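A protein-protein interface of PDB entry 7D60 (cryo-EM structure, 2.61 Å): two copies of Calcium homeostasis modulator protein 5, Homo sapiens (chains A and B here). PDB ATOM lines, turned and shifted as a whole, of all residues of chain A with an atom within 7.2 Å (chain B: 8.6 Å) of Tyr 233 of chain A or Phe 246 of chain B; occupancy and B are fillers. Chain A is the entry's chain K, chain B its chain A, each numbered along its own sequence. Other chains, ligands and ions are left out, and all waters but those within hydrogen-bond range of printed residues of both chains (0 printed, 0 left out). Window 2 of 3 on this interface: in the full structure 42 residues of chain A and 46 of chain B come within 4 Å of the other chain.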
ATOM      1  N   GLN A 225      21.326   1.459 -12.670  1.00  0.00           N
ATOM      2  CA  GLN A 225      21.905   2.562 -13.418  1.00  0.00           C
ATOM      3  C   GLN A 225      20.870   3.609 -13.780  1.00  0.00           C
ATOM      4  O   GLN A 225      21.233   4.763 -14.016  1.00  0.00           O
ATOM      5  CB  GLN A 225      22.574   2.038 -14.684  1.00  0.00           C
ATOM      6  CG  GLN A 225      23.818   1.223 -14.435  1.00  0.00           C
ATOM      7  CD  GLN A 225      25.016   2.081 -14.153  1.00  0.00           C
ATOM      8  OE1 GLN A 225      25.480   2.170 -13.018  1.00  0.00           O
ATOM      9  NE2 GLN A 225      25.528   2.725 -15.185  1.00  0.00           N
ATOM     10  N   LEU A 226      19.594   3.234 -13.826  1.00  0.00           N
ATOM     11  CA  LEU A 226      18.533   4.192 -14.093  1.00  0.00           C
ATOM     12  C   LEU A 226      18.207   5.027 -12.867  1.00  0.00           C
ATOM     13  O   LEU A 226      17.774   6.170 -13.005  1.00  0.00           O
ATOM     14  CB  LEU A 226      17.288   3.457 -14.576  1.00  0.00           C
ATOM     15  CG  LEU A 226      16.187   4.202 -15.307  1.00  0.00           C
ATOM     16  CD1 LEU A 226      16.764   5.006 -16.437  1.00  0.00           C
ATOM     17  CD2 LEU A 226      15.219   3.191 -15.845  1.00  0.00           C
ATOM     18  N   ASN A 228      20.503   6.014 -10.754  1.00  0.00           N
ATOM     19  CA  ASN A 228      21.598   6.963 -10.625  1.00  0.00           C
ATOM     20  C   ASN A 228      21.579   8.030 -11.706  1.00  0.00           C
ATOM     21  O   ASN A 228      22.145   9.104 -11.502  1.00  0.00           O
ATOM     22  CB  ASN A 228      22.935   6.228 -10.655  1.00  0.00           C
ATOM     23  CG  ASN A 228      23.091   5.261  -9.507  1.00  0.00           C
ATOM     24  OD1 ASN A 228      22.400   5.365  -8.497  1.00  0.00           O
ATOM     25  ND2 ASN A 228      24.003   4.312  -9.654  1.00  0.00           N
ATOM     26  N   THR A 229      20.955   7.761 -12.848  1.00  0.00           N
ATOM     27  CA  THR A 229      20.829   8.779 -13.880  1.00  0.00           C
ATOM     28  C   THR A 229      19.691   9.738 -13.566  1.00  0.00           C
ATOM     29  O   THR A 229      19.804  10.941 -13.820  1.00  0.00           O
ATOM     30  CB  THR A 229      20.622   8.112 -15.238  1.00  0.00           C
ATOM     31  OG1 THR A 229      21.667   7.163 -15.449  1.00  0.00           O
ATOM     32  CG2 THR A 229      20.666   9.122 -16.359  1.00  0.00           C
ATOM     33  N   PHE A 230      18.596   9.225 -13.003  1.00  0.00           N
ATOM     34  CA  PHE A 230      17.493  10.083 -12.585  1.00  0.00           C
ATOM     35  C   PHE A 230      17.914  10.992 -11.443  1.00  0.00           C
ATOM     36  O   PHE A 230      17.541  12.165 -11.406  1.00  0.00           O
ATOM     37  CB  PHE A 230      16.296   9.239 -12.155  1.00  0.00           C
ATOM     38  CG  PHE A 230      15.497   8.684 -13.291  1.00  0.00           C
ATOM     39  CD1 PHE A 230      15.762   9.041 -14.597  1.00  0.00           C
ATOM     40  CD2 PHE A 230      14.472   7.797 -13.044  1.00  0.00           C
ATOM     41  CE1 PHE A 230      15.020   8.524 -15.626  1.00  0.00           C
ATOM     42  CE2 PHE A 230      13.731   7.281 -14.073  1.00  0.00           C
ATOM     43  CZ  PHE A 230      14.005   7.646 -15.363  1.00  0.00           C
ATOM     44  N   LEU A 231      18.707  10.469 -10.519  1.00  0.00           N
ATOM     45  CA  LEU A 231      19.183  11.233  -9.377  1.00  0.00           C
ATOM     46  C   LEU A 231      20.248  12.249  -9.764  1.00  0.00           C
ATOM     47  O   LEU A 231      20.496  13.189  -9.007  1.00  0.00           O
ATOM     48  CB  LEU A 231      19.720  10.262  -8.329  1.00  0.00           C
ATOM     49  CG  LEU A 231      19.911  10.612  -6.864  1.00  0.00           C
ATOM     50  CD1 LEU A 231      19.566   9.403  -6.031  1.00  0.00           C
ATOM     51  CD2 LEU A 231      21.337  11.040  -6.600  1.00  0.00           C
ATOM     52  N   ASP A 232      20.872  12.085 -10.925  1.00  0.00           N
ATOM     53  CA  ASP A 232      21.896  13.009 -11.388  1.00  0.00           C
ATOM     54  C   ASP A 232      21.312  14.121 -12.247  1.00  0.00           C
ATOM     55  O   ASP A 232      21.767  15.264 -12.166  1.00  0.00           O
ATOM     56  CB  ASP A 232      22.959  12.229 -12.160  1.00  0.00           C
ATOM     57  CG  ASP A 232      23.971  13.117 -12.827  1.00  0.00           C
ATOM     58  OD1 ASP A 232      24.750  13.775 -12.109  1.00  0.00           O
ATOM     59  OD2 ASP A 232      24.002  13.145 -14.075  1.00  0.00           O
ATOM     60  N   TYR A 233      20.309  13.814 -13.065  1.00  0.00           N
ATOM     61  CA  TYR A 233      19.666  14.825 -13.888  1.00  0.00           C
ATOM     62  C   TYR A 233      18.634  15.636 -13.123  1.00  0.00           C
ATOM     63  O   TYR A 233      18.176  16.659 -13.634  1.00  0.00           O
ATOM     64  CB  TYR A 233      18.992  14.177 -15.091  1.00  0.00           C
ATOM     65  CG  TYR A 233      19.880  14.047 -16.292  1.00  0.00           C
ATOM     66  CD1 TYR A 233      19.718  14.877 -17.389  1.00  0.00           C
ATOM     67  CD2 TYR A 233      20.878  13.088 -16.337  1.00  0.00           C
ATOM     68  CE1 TYR A 233      20.528  14.758 -18.493  1.00  0.00           C
ATOM     69  CE2 TYR A 233      21.692  12.961 -17.434  1.00  0.00           C
ATOM     70  CZ  TYR A 233      21.513  13.797 -18.509  1.00  0.00           C
ATOM     71  OH  TYR A 233      22.327  13.671 -19.607  1.00  0.00           O
ATOM     72  N   ALA A 234      18.245  15.201 -11.928  1.00  0.00           N
ATOM     73  CA  ALA A 234      17.306  15.982 -11.137  1.00  0.00           C
ATOM     74  C   ALA A 234      18.020  16.923 -10.183  1.00  0.00           C
ATOM     75  O   ALA A 234      17.428  17.909  -9.741  1.00  0.00           O
ATOM     76  CB  ALA A 234      16.364  15.063 -10.368  1.00  0.00           C
ATOM     77  N   ASN A 235      19.278  16.640  -9.853  1.00  0.00           N
ATOM     78  CA  ASN A 235      20.093  17.611  -9.137  1.00  0.00           C
ATOM     79  C   ASN A 235      20.503  18.769 -10.028  1.00  0.00           C
ATOM     80  O   ASN A 235      20.587  19.904  -9.557  1.00  0.00           O
ATOM     81  CB  ASN A 235      21.343  16.949  -8.569  1.00  0.00           C
ATOM     82  CG  ASN A 235      21.182  16.550  -7.131  1.00  0.00           C
ATOM     83  OD1 ASN A 235      20.585  17.273  -6.342  1.00  0.00           O
ATOM     84  ND2 ASN A 235      21.731  15.402  -6.772  1.00  0.00           N
ATOM     85  N   LYS A 236      20.765  18.508 -11.302  1.00  0.00           N
ATOM     86  CA  LYS A 236      21.155  19.566 -12.216  1.00  0.00           C
ATOM     87  C   LYS A 236      19.982  20.423 -12.650  1.00  0.00           C
ATOM     88  O   LYS A 236      20.186  21.581 -13.018  1.00  0.00           O
ATOM     89  CB  LYS A 236      21.833  18.973 -13.448  1.00  0.00           C
ATOM     90  CG  LYS A 236      23.263  18.541 -13.217  1.00  0.00           C
ATOM     91  CD  LYS A 236      23.693  17.505 -14.232  1.00  0.00           C
ATOM     92  CE  LYS A 236      23.559  18.029 -15.647  1.00  0.00           C
ATOM     93  NZ  LYS A 236      23.605  16.931 -16.648  1.00  0.00           N
ATOM     94  N   LEU A 237      18.768  19.886 -12.624  1.00  0.00           N
ATOM     95  CA  LEU A 237      17.591  20.657 -12.995  1.00  0.00           C
ATOM     96  C   LEU A 237      17.088  21.517 -11.846  1.00  0.00           C
ATOM     97  O   LEU A 237      16.617  22.633 -12.073  1.00  0.00           O
ATOM     98  CB  LEU A 237      16.483  19.720 -13.474  1.00  0.00           C
ATOM     99  CG  LEU A 237      15.196  20.348 -13.999  1.00  0.00           C
ATOM    100  CD1 LEU A 237      15.502  21.333 -15.101  1.00  0.00           C
ATOM    101  CD2 LEU A 237      14.248  19.282 -14.485  1.00  0.00           C
ATOM    102  N   SER A 238      17.188  21.030 -10.611  1.00  0.00           N
ATOM    103  CA  SER A 238      16.739  21.826  -9.477  1.00  0.00           C
ATOM    104  C   SER A 238      17.729  22.927  -9.128  1.00  0.00           C
ATOM    105  O   SER A 238      17.329  23.960  -8.587  1.00  0.00           O
ATOM    106  CB  SER A 238      16.493  20.928  -8.269  1.00  0.00           C
ATOM    107  OG  SER A 238      17.700  20.630  -7.606  1.00  0.00           O
ATOM    108  N   PHE A 254      17.805  23.279 -21.152  1.00  0.00           N
ATOM    109  CA  PHE A 254      18.098  21.991 -20.522  1.00  0.00           C
ATOM    110  C   PHE A 254      17.564  20.881 -21.409  1.00  0.00           C
ATOM    111  O   PHE A 254      16.334  20.704 -21.494  1.00  0.00           O
ATOM    112  CB  PHE A 254      17.460  21.924 -19.136  1.00  0.00           C
ATOM    113  CG  PHE A 254      18.086  20.921 -18.220  1.00  0.00           C
ATOM    114  CD1 PHE A 254      19.269  21.204 -17.567  1.00  0.00           C
ATOM    115  CD2 PHE A 254      17.477  19.701 -17.994  1.00  0.00           C
ATOM    116  CE1 PHE A 254      19.843  20.285 -16.715  1.00  0.00           C
ATOM    117  CE2 PHE A 254      18.046  18.777 -17.144  1.00  0.00           C
ATOM    118  CZ  PHE A 254      19.229  19.069 -16.505  1.00  0.00           C
ATOM    119  N   PRO A 255      18.418  20.118 -22.092  1.00  0.00           N
ATOM    120  CA  PRO A 255      17.916  19.103 -23.031  1.00  0.00           C
ATOM    121  C   PRO A 255      17.412  17.859 -22.308  1.00  0.00           C
ATOM    122  O   PRO A 255      18.128  17.241 -21.518  1.00  0.00           O
ATOM    123  CB  PRO A 255      19.137  18.790 -23.902  1.00  0.00           C
ATOM    124  CG  PRO A 255      20.308  19.167 -23.074  1.00  0.00           C
ATOM    125  CD  PRO A 255      19.882  20.252 -22.136  1.00  0.00           C
ATOM    126  N   MET A 256      16.171  17.496 -22.594  1.00  0.00           N
ATOM    127  CA  MET A 256      15.487  16.340 -22.042  1.00  0.00           C
ATOM    128  C   MET A 256      14.900  15.544 -23.195  1.00  0.00           C
ATOM    129  O   MET A 256      14.693  16.090 -24.284  1.00  0.00           O
ATOM    130  CB  MET A 256      14.369  16.770 -21.079  1.00  0.00           C
ATOM    131  CG  MET A 256      14.847  17.453 -19.818  1.00  0.00           C
ATOM    132  SD  MET A 256      15.869  16.384 -18.802  1.00  0.00           S
ATOM    133  CE  MET A 256      14.619  15.352 -18.063  1.00  0.00           C
ATOM    134  N   PRO A 257      14.649  14.246 -23.004  1.00  0.00           N
ATOM    135  CA  PRO A 257      13.952  13.478 -24.043  1.00  0.00           C
ATOM    136  C   PRO A 257      12.522  13.957 -24.231  1.00  0.00           C
ATOM    137  O   PRO A 257      11.875  14.431 -23.300  1.00  0.00           O
ATOM    138  CB  PRO A 257      13.997  12.038 -23.520  1.00  0.00           C
ATOM    139  CG  PRO A 257      14.455  12.119 -22.126  1.00  0.00           C
ATOM    140  CD  PRO A 257      15.241  13.364 -21.986  1.00  0.00           C
ATOM    141  N   TRP A 262       9.703   9.241 -24.289  1.00  0.00           N
ATOM    142  CA  TRP A 262       9.376   8.733 -22.962  1.00  0.00           C
ATOM    143  C   TRP A 262       8.340   7.622 -23.042  1.00  0.00           C
ATOM    144  O   TRP A 262       8.412   6.646 -22.290  1.00  0.00           O
ATOM    145  CB  TRP A 262       8.845   9.857 -22.080  1.00  0.00           C
ATOM    146  CG  TRP A 262       9.847  10.710 -21.369  1.00  0.00           C
ATOM    147  CD1 TRP A 262      10.043  12.039 -21.549  1.00  0.00           C
ATOM    148  CD2 TRP A 262      10.737  10.316 -20.325  1.00  0.00           C
ATOM    149  NE1 TRP A 262      11.014  12.496 -20.709  1.00  0.00           N
ATOM    150  CE2 TRP A 262      11.456  11.456 -19.941  1.00  0.00           C
ATOM    151  CE3 TRP A 262      11.004   9.107 -19.686  1.00  0.00           C
ATOM    152  CZ2 TRP A 262      12.420  11.427 -18.949  1.00  0.00           C
ATOM    153  CZ3 TRP A 262      11.965   9.082 -18.705  1.00  0.00           C
ATOM    154  CH2 TRP A 262      12.660  10.233 -18.345  1.00  0.00           C
ATOM    155  N   LEU A 281      14.188  -0.432 -23.668  1.00  0.00           N
ATOM    156  CA  LEU A 281      15.083   0.707 -23.792  1.00  0.00           C
ATOM    157  C   LEU A 281      16.274   0.386 -24.679  1.00  0.00           C
ATOM    158  O   LEU A 281      16.802   1.277 -25.345  1.00  0.00           O
ATOM    159  CB  LEU A 281      15.556   1.146 -22.411  1.00  0.00           C
ATOM    160  CG  LEU A 281      16.248   2.494 -22.293  1.00  0.00           C
ATOM    161  CD1 LEU A 281      15.392   3.562 -22.905  1.00  0.00           C
ATOM    162  CD2 LEU A 281      16.499   2.797 -20.845  1.00  0.00           C
ATOM    163  N   VAL A 285      16.897   2.468 -28.602  1.00  0.00           N
ATOM    164  CA  VAL A 285      18.194   3.080 -28.864  1.00  0.00           C
ATOM    165  C   VAL A 285      18.810   2.509 -30.135  1.00  0.00           C
ATOM    166  O   VAL A 285      19.318   3.253 -30.980  1.00  0.00           O
ATOM    167  CB  VAL A 285      19.107   2.900 -27.639  1.00  0.00           C
ATOM    168  CG1 VAL A 285      20.532   3.267 -27.955  1.00  0.00           C
ATOM    169  CG2 VAL A 285      18.614   3.767 -26.513  1.00  0.00           C
ATOM    170  N   ARG B 240      25.876   2.271 -22.025  1.00  0.00           N
ATOM    171  CA  ARG B 240      25.750   2.720 -23.404  1.00  0.00           C
ATOM    172  C   ARG B 240      24.320   3.121 -23.727  1.00  0.00           C
ATOM    173  O   ARG B 240      24.093   4.117 -24.418  1.00  0.00           O
ATOM    174  CB  ARG B 240      26.219   1.618 -24.348  1.00  0.00           C
ATOM    175  CG  ARG B 240      26.227   1.995 -25.805  1.00  0.00           C
ATOM    176  CD  ARG B 240      26.290   0.761 -26.667  1.00  0.00           C
ATOM    177  NE  ARG B 240      24.963   0.225 -26.935  1.00  0.00           N
ATOM    178  CZ  ARG B 240      24.483   0.005 -28.151  1.00  0.00           C
ATOM    179  NH1 ARG B 240      25.226   0.260 -29.211  1.00  0.00           N
ATOM    180  NH2 ARG B 240      23.264  -0.480 -28.307  1.00  0.00           N
ATOM    181  N   ASN B 241      23.345   2.362 -23.235  1.00  0.00           N
ATOM    182  CA  ASN B 241      21.956   2.597 -23.602  1.00  0.00           C
ATOM    183  C   ASN B 241      21.375   3.818 -22.910  1.00  0.00           C
ATOM    184  O   ASN B 241      20.431   4.420 -23.426  1.00  0.00           O
ATOM    185  CB  ASN B 241      21.113   1.369 -23.273  1.00  0.00           C
ATOM    186  CG  ASN B 241      21.331   0.244 -24.243  1.00  0.00           C
ATOM    187  OD1 ASN B 241      21.810   0.450 -25.350  1.00  0.00           O
ATOM    188  ND2 ASN B 241      20.979  -0.959 -23.834  1.00  0.00           N
ATOM    189  N   LEU B 242      21.915   4.202 -21.762  1.00  0.00           N
ATOM    190  CA  LEU B 242      21.376   5.337 -21.032  1.00  0.00           C
ATOM    191  C   LEU B 242      21.936   6.668 -21.502  1.00  0.00           C
ATOM    192  O   LEU B 242      21.242   7.684 -21.417  1.00  0.00           O
ATOM    193  CB  LEU B 242      21.646   5.173 -19.539  1.00  0.00           C
ATOM    194  CG  LEU B 242      20.761   4.123 -18.887  1.00  0.00           C
ATOM    195  CD1 LEU B 242      21.098   3.995 -17.439  1.00  0.00           C
ATOM    196  CD2 LEU B 242      19.326   4.508 -19.062  1.00  0.00           C
ATOM    197  N   LYS B 243      23.172   6.692 -21.989  1.00  0.00           N
ATOM    198  CA  LYS B 243      23.725   7.926 -22.524  1.00  0.00           C
ATOM    199  C   LYS B 243      23.122   8.284 -23.870  1.00  0.00           C
ATOM    200  O   LYS B 243      23.005   9.467 -24.192  1.00  0.00           O
ATOM    201  CB  LYS B 243      25.241   7.812 -22.652  1.00  0.00           C
ATOM    202  CG  LYS B 243      25.975   7.912 -21.336  1.00  0.00           C
ATOM    203  CD  LYS B 243      27.474   7.907 -21.549  1.00  0.00           C
ATOM    204  CE  LYS B 243      27.926   6.646 -22.265  1.00  0.00           C
ATOM    205  NZ  LYS B 243      29.407   6.541 -22.321  1.00  0.00           N
ATOM    206  N   CYS B 244      22.736   7.297 -24.665  1.00  0.00           N
ATOM    207  CA  CYS B 244      22.145   7.564 -25.965  1.00  0.00           C
ATOM    208  C   CYS B 244      20.644   7.789 -25.897  1.00  0.00           C
ATOM    209  O   CYS B 244      20.025   8.045 -26.933  1.00  0.00           O
ATOM    210  CB  CYS B 244      22.451   6.419 -26.927  1.00  0.00           C
ATOM    211  SG  CYS B 244      24.203   6.036 -27.071  1.00  0.00           S
ATOM    212  N   PHE B 245      20.043   7.690 -24.717  1.00  0.00           N
ATOM    213  CA  PHE B 245      18.629   7.994 -24.558  1.00  0.00           C
ATOM    214  C   PHE B 245      18.413   9.424 -24.092  1.00  0.00           C
ATOM    215  O   PHE B 245      17.560  10.131 -24.635  1.00  0.00           O
ATOM    216  CB  PHE B 245      17.985   7.016 -23.574  1.00  0.00           C
ATOM    217  CG  PHE B 245      16.531   7.276 -23.325  1.00  0.00           C
ATOM    218  CD1 PHE B 245      15.603   7.115 -24.336  1.00  0.00           C
ATOM    219  CD2 PHE B 245      16.091   7.682 -22.080  1.00  0.00           C
ATOM    220  CE1 PHE B 245      14.268   7.358 -24.107  1.00  0.00           C
ATOM    221  CE2 PHE B 245      14.757   7.927 -21.849  1.00  0.00           C
ATOM    222  CZ  PHE B 245      13.847   7.765 -22.863  1.00  0.00           C
ATOM    223  N   PHE B 246      19.190   9.870 -23.108  1.00  0.00           N
ATOM    224  CA  PHE B 246      19.013  11.211 -22.571  1.00  0.00           C
ATOM    225  C   PHE B 246      19.620  12.278 -23.465  1.00  0.00           C
ATOM    226  O   PHE B 246      19.082  13.385 -23.552  1.00  0.00           O
ATOM    227  CB  PHE B 246      19.620  11.292 -21.179  1.00  0.00           C
ATOM    228  CG  PHE B 246      18.713  10.800 -20.111  1.00  0.00           C
ATOM    229  CD1 PHE B 246      17.809  11.657 -19.509  1.00  0.00           C
ATOM    230  CD2 PHE B 246      18.748   9.477 -19.718  1.00  0.00           C
ATOM    231  CE1 PHE B 246      16.966  11.208 -18.528  1.00  0.00           C
ATOM    232  CE2 PHE B 246      17.903   9.018 -18.737  1.00  0.00           C
ATOM    233  CZ  PHE B 246      17.012   9.887 -18.141  1.00  0.00           C
ATOM    234  N   GLU B 247      20.726  11.970 -24.132  1.00  0.00           N
ATOM    235  CA  GLU B 247      21.403  12.928 -24.987  1.00  0.00           C
ATOM    236  C   GLU B 247      20.955  12.860 -26.438  1.00  0.00           C
ATOM    237  O   GLU B 247      21.403  13.690 -27.235  1.00  0.00           O
ATOM    238  CB  GLU B 247      22.916  12.721 -24.904  1.00  0.00           C
ATOM    239  CG  GLU B 247      23.425  12.725 -23.479  1.00  0.00           C
ATOM    240  CD  GLU B 247      24.875  12.326 -23.371  1.00  0.00           C
ATOM    241  OE1 GLU B 247      25.501  12.059 -24.415  1.00  0.00           O
ATOM    242  OE2 GLU B 247      25.393  12.277 -22.239  1.00  0.00           O
ATOM    243  N   ASN B 248      20.084  11.903 -26.778  1.00  0.00           N
ATOM    244  CA  ASN B 248      19.541  11.695 -28.126  1.00  0.00           C
ATOM    245  C   ASN B 248      20.649  11.484 -29.158  1.00  0.00           C
ATOM    246  O   ASN B 248      20.665  12.096 -30.227  1.00  0.00           O
ATOM    247  CB  ASN B 248      18.609  12.839 -28.536  1.00  0.00           C
ATOM    248  CG  ASN B 248      17.618  12.424 -29.599  1.00  0.00           C
ATOM    249  OD1 ASN B 248      17.364  11.239 -29.800  1.00  0.00           O
ATOM    250  ND2 ASN B 248      17.053  13.403 -30.293  1.00  0.00           N
ATOM    251  N   LYS B 249      21.584  10.605 -28.825  1.00  0.00           N
ATOM    252  CA  LYS B 249      22.705  10.276 -29.689  1.00  0.00           C
ATOM    253  C   LYS B 249      22.465   8.957 -30.408  1.00  0.00           C
ATOM    254  O   LYS B 249      21.592   8.168 -30.042  1.00  0.00           O
ATOM    255  CB  LYS B 249      24.000  10.187 -28.884  1.00  0.00           C
ATOM    256  CG  LYS B 249      24.717  11.502 -28.722  1.00  0.00           C
ATOM    257  CD  LYS B 249      25.813  11.387 -27.687  1.00  0.00           C
ATOM    258  CE  LYS B 249      26.549  12.702 -27.521  1.00  0.00           C
ATOM    259  NZ  LYS B 249      27.213  12.783 -26.191  1.00  0.00           N
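The side-chain amide oxygen (OD1) of Asn 241 of chain B sits at hydrogen-bond distance from the guanidinium group (NH2) of Arg 240 of chain B (3.4 Å).
The backbone carbonyl oxygen (O) of Arg 240 of chain B lies within hydrogen-bond range of the side-chain sulfur (SG) of Cys 244 of chain B.
The backbone carbonyl oxygen (O) of Gln 225 of chain A is in hydrogen-bond range of the side-chain hydroxyl (OG1) of Thr 229 of chain A (2.8 Å).
NE1 of Trp 262 of chain A lies within hydrogen-bond range of O of Pro 257 of chain A (3.3 Å).
Among the printed residues, merely in contact across the chains: Phe 230 of chain A with Phe 246 of chain B (3.5 Å), Gln 225 of chain A with Leu 242 of chain B (3.5 Å), Val 285 of chain A with Asn 241 of chain B (3.6 Å), Thr 229 of chain A with Phe 246 of chain B (3.6 Å), Leu 226 of chain A with Leu 242 of chain B (3.7 Å), Leu 281 of chain A with Leu 242 of chain B (3.8 Å), Thr 229 of chain A with Leu 242 of chain B (3.8 Å), Val 285 of chain A with Cys 244 of chain B (3.8 Å), Leu 281 of chain A with Phe 245 of chain B (3.8 Å), Tyr 233 of chain A with Phe 246 of chain B (3.9 Å) and Pro 257 of chain A with Phe 246 of chain B (3.96 Å).
Of chain A, only Thr 229, Phe 230, Tyr 233 and Pro 257 come within 4 Å of Phe 246 of chain B.
No residue of chain B comes within 4 Å of Ala 234 of chain A.
Of the printed residues of chain A, Asn 241 of chain B touches Val 285 (3.6 Å).
Printed residues of chain A within 4 Å of Leu 242 of chain B: Gln 225 (3.5 Å), Leu 226 (3.7 Å), Thr 229 (3.8 Å) and Leu 281 (3.8 Å).
Of the printed residues of chain B, Val 285 of chain A touches Asn 241 and Cys 244.
Of the 10 printed residues of chain B, 5 touch a printed residue of chain A.
Printed residues of chain B that touch a printed residue of chain A: Asn 241, Leu 242, Cys 244, Phe 245 and Phe 246.
Hydrophobic or aromatic side chains of chain B within 4 Å of the printed part of chain A: Leu 242, Phe 245 and Phe 246.
Of the 20 printed residues of chain A, 8 touch a printed residue of chain B.
Hydrophobic or aromatic side chains of chain A within 4 Å of the printed part of chain B: Leu 226, Phe 230, Tyr 233, Pro 257, Leu 281 and Val 285.
Among the printed residues, 11 pairs touch across the chains.
Among the printed residues, no Asp or Glu carboxylate lies within 4 Å of a Lys or Arg side-chain nitrogen of the other chain.
No position is printed for both chains.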
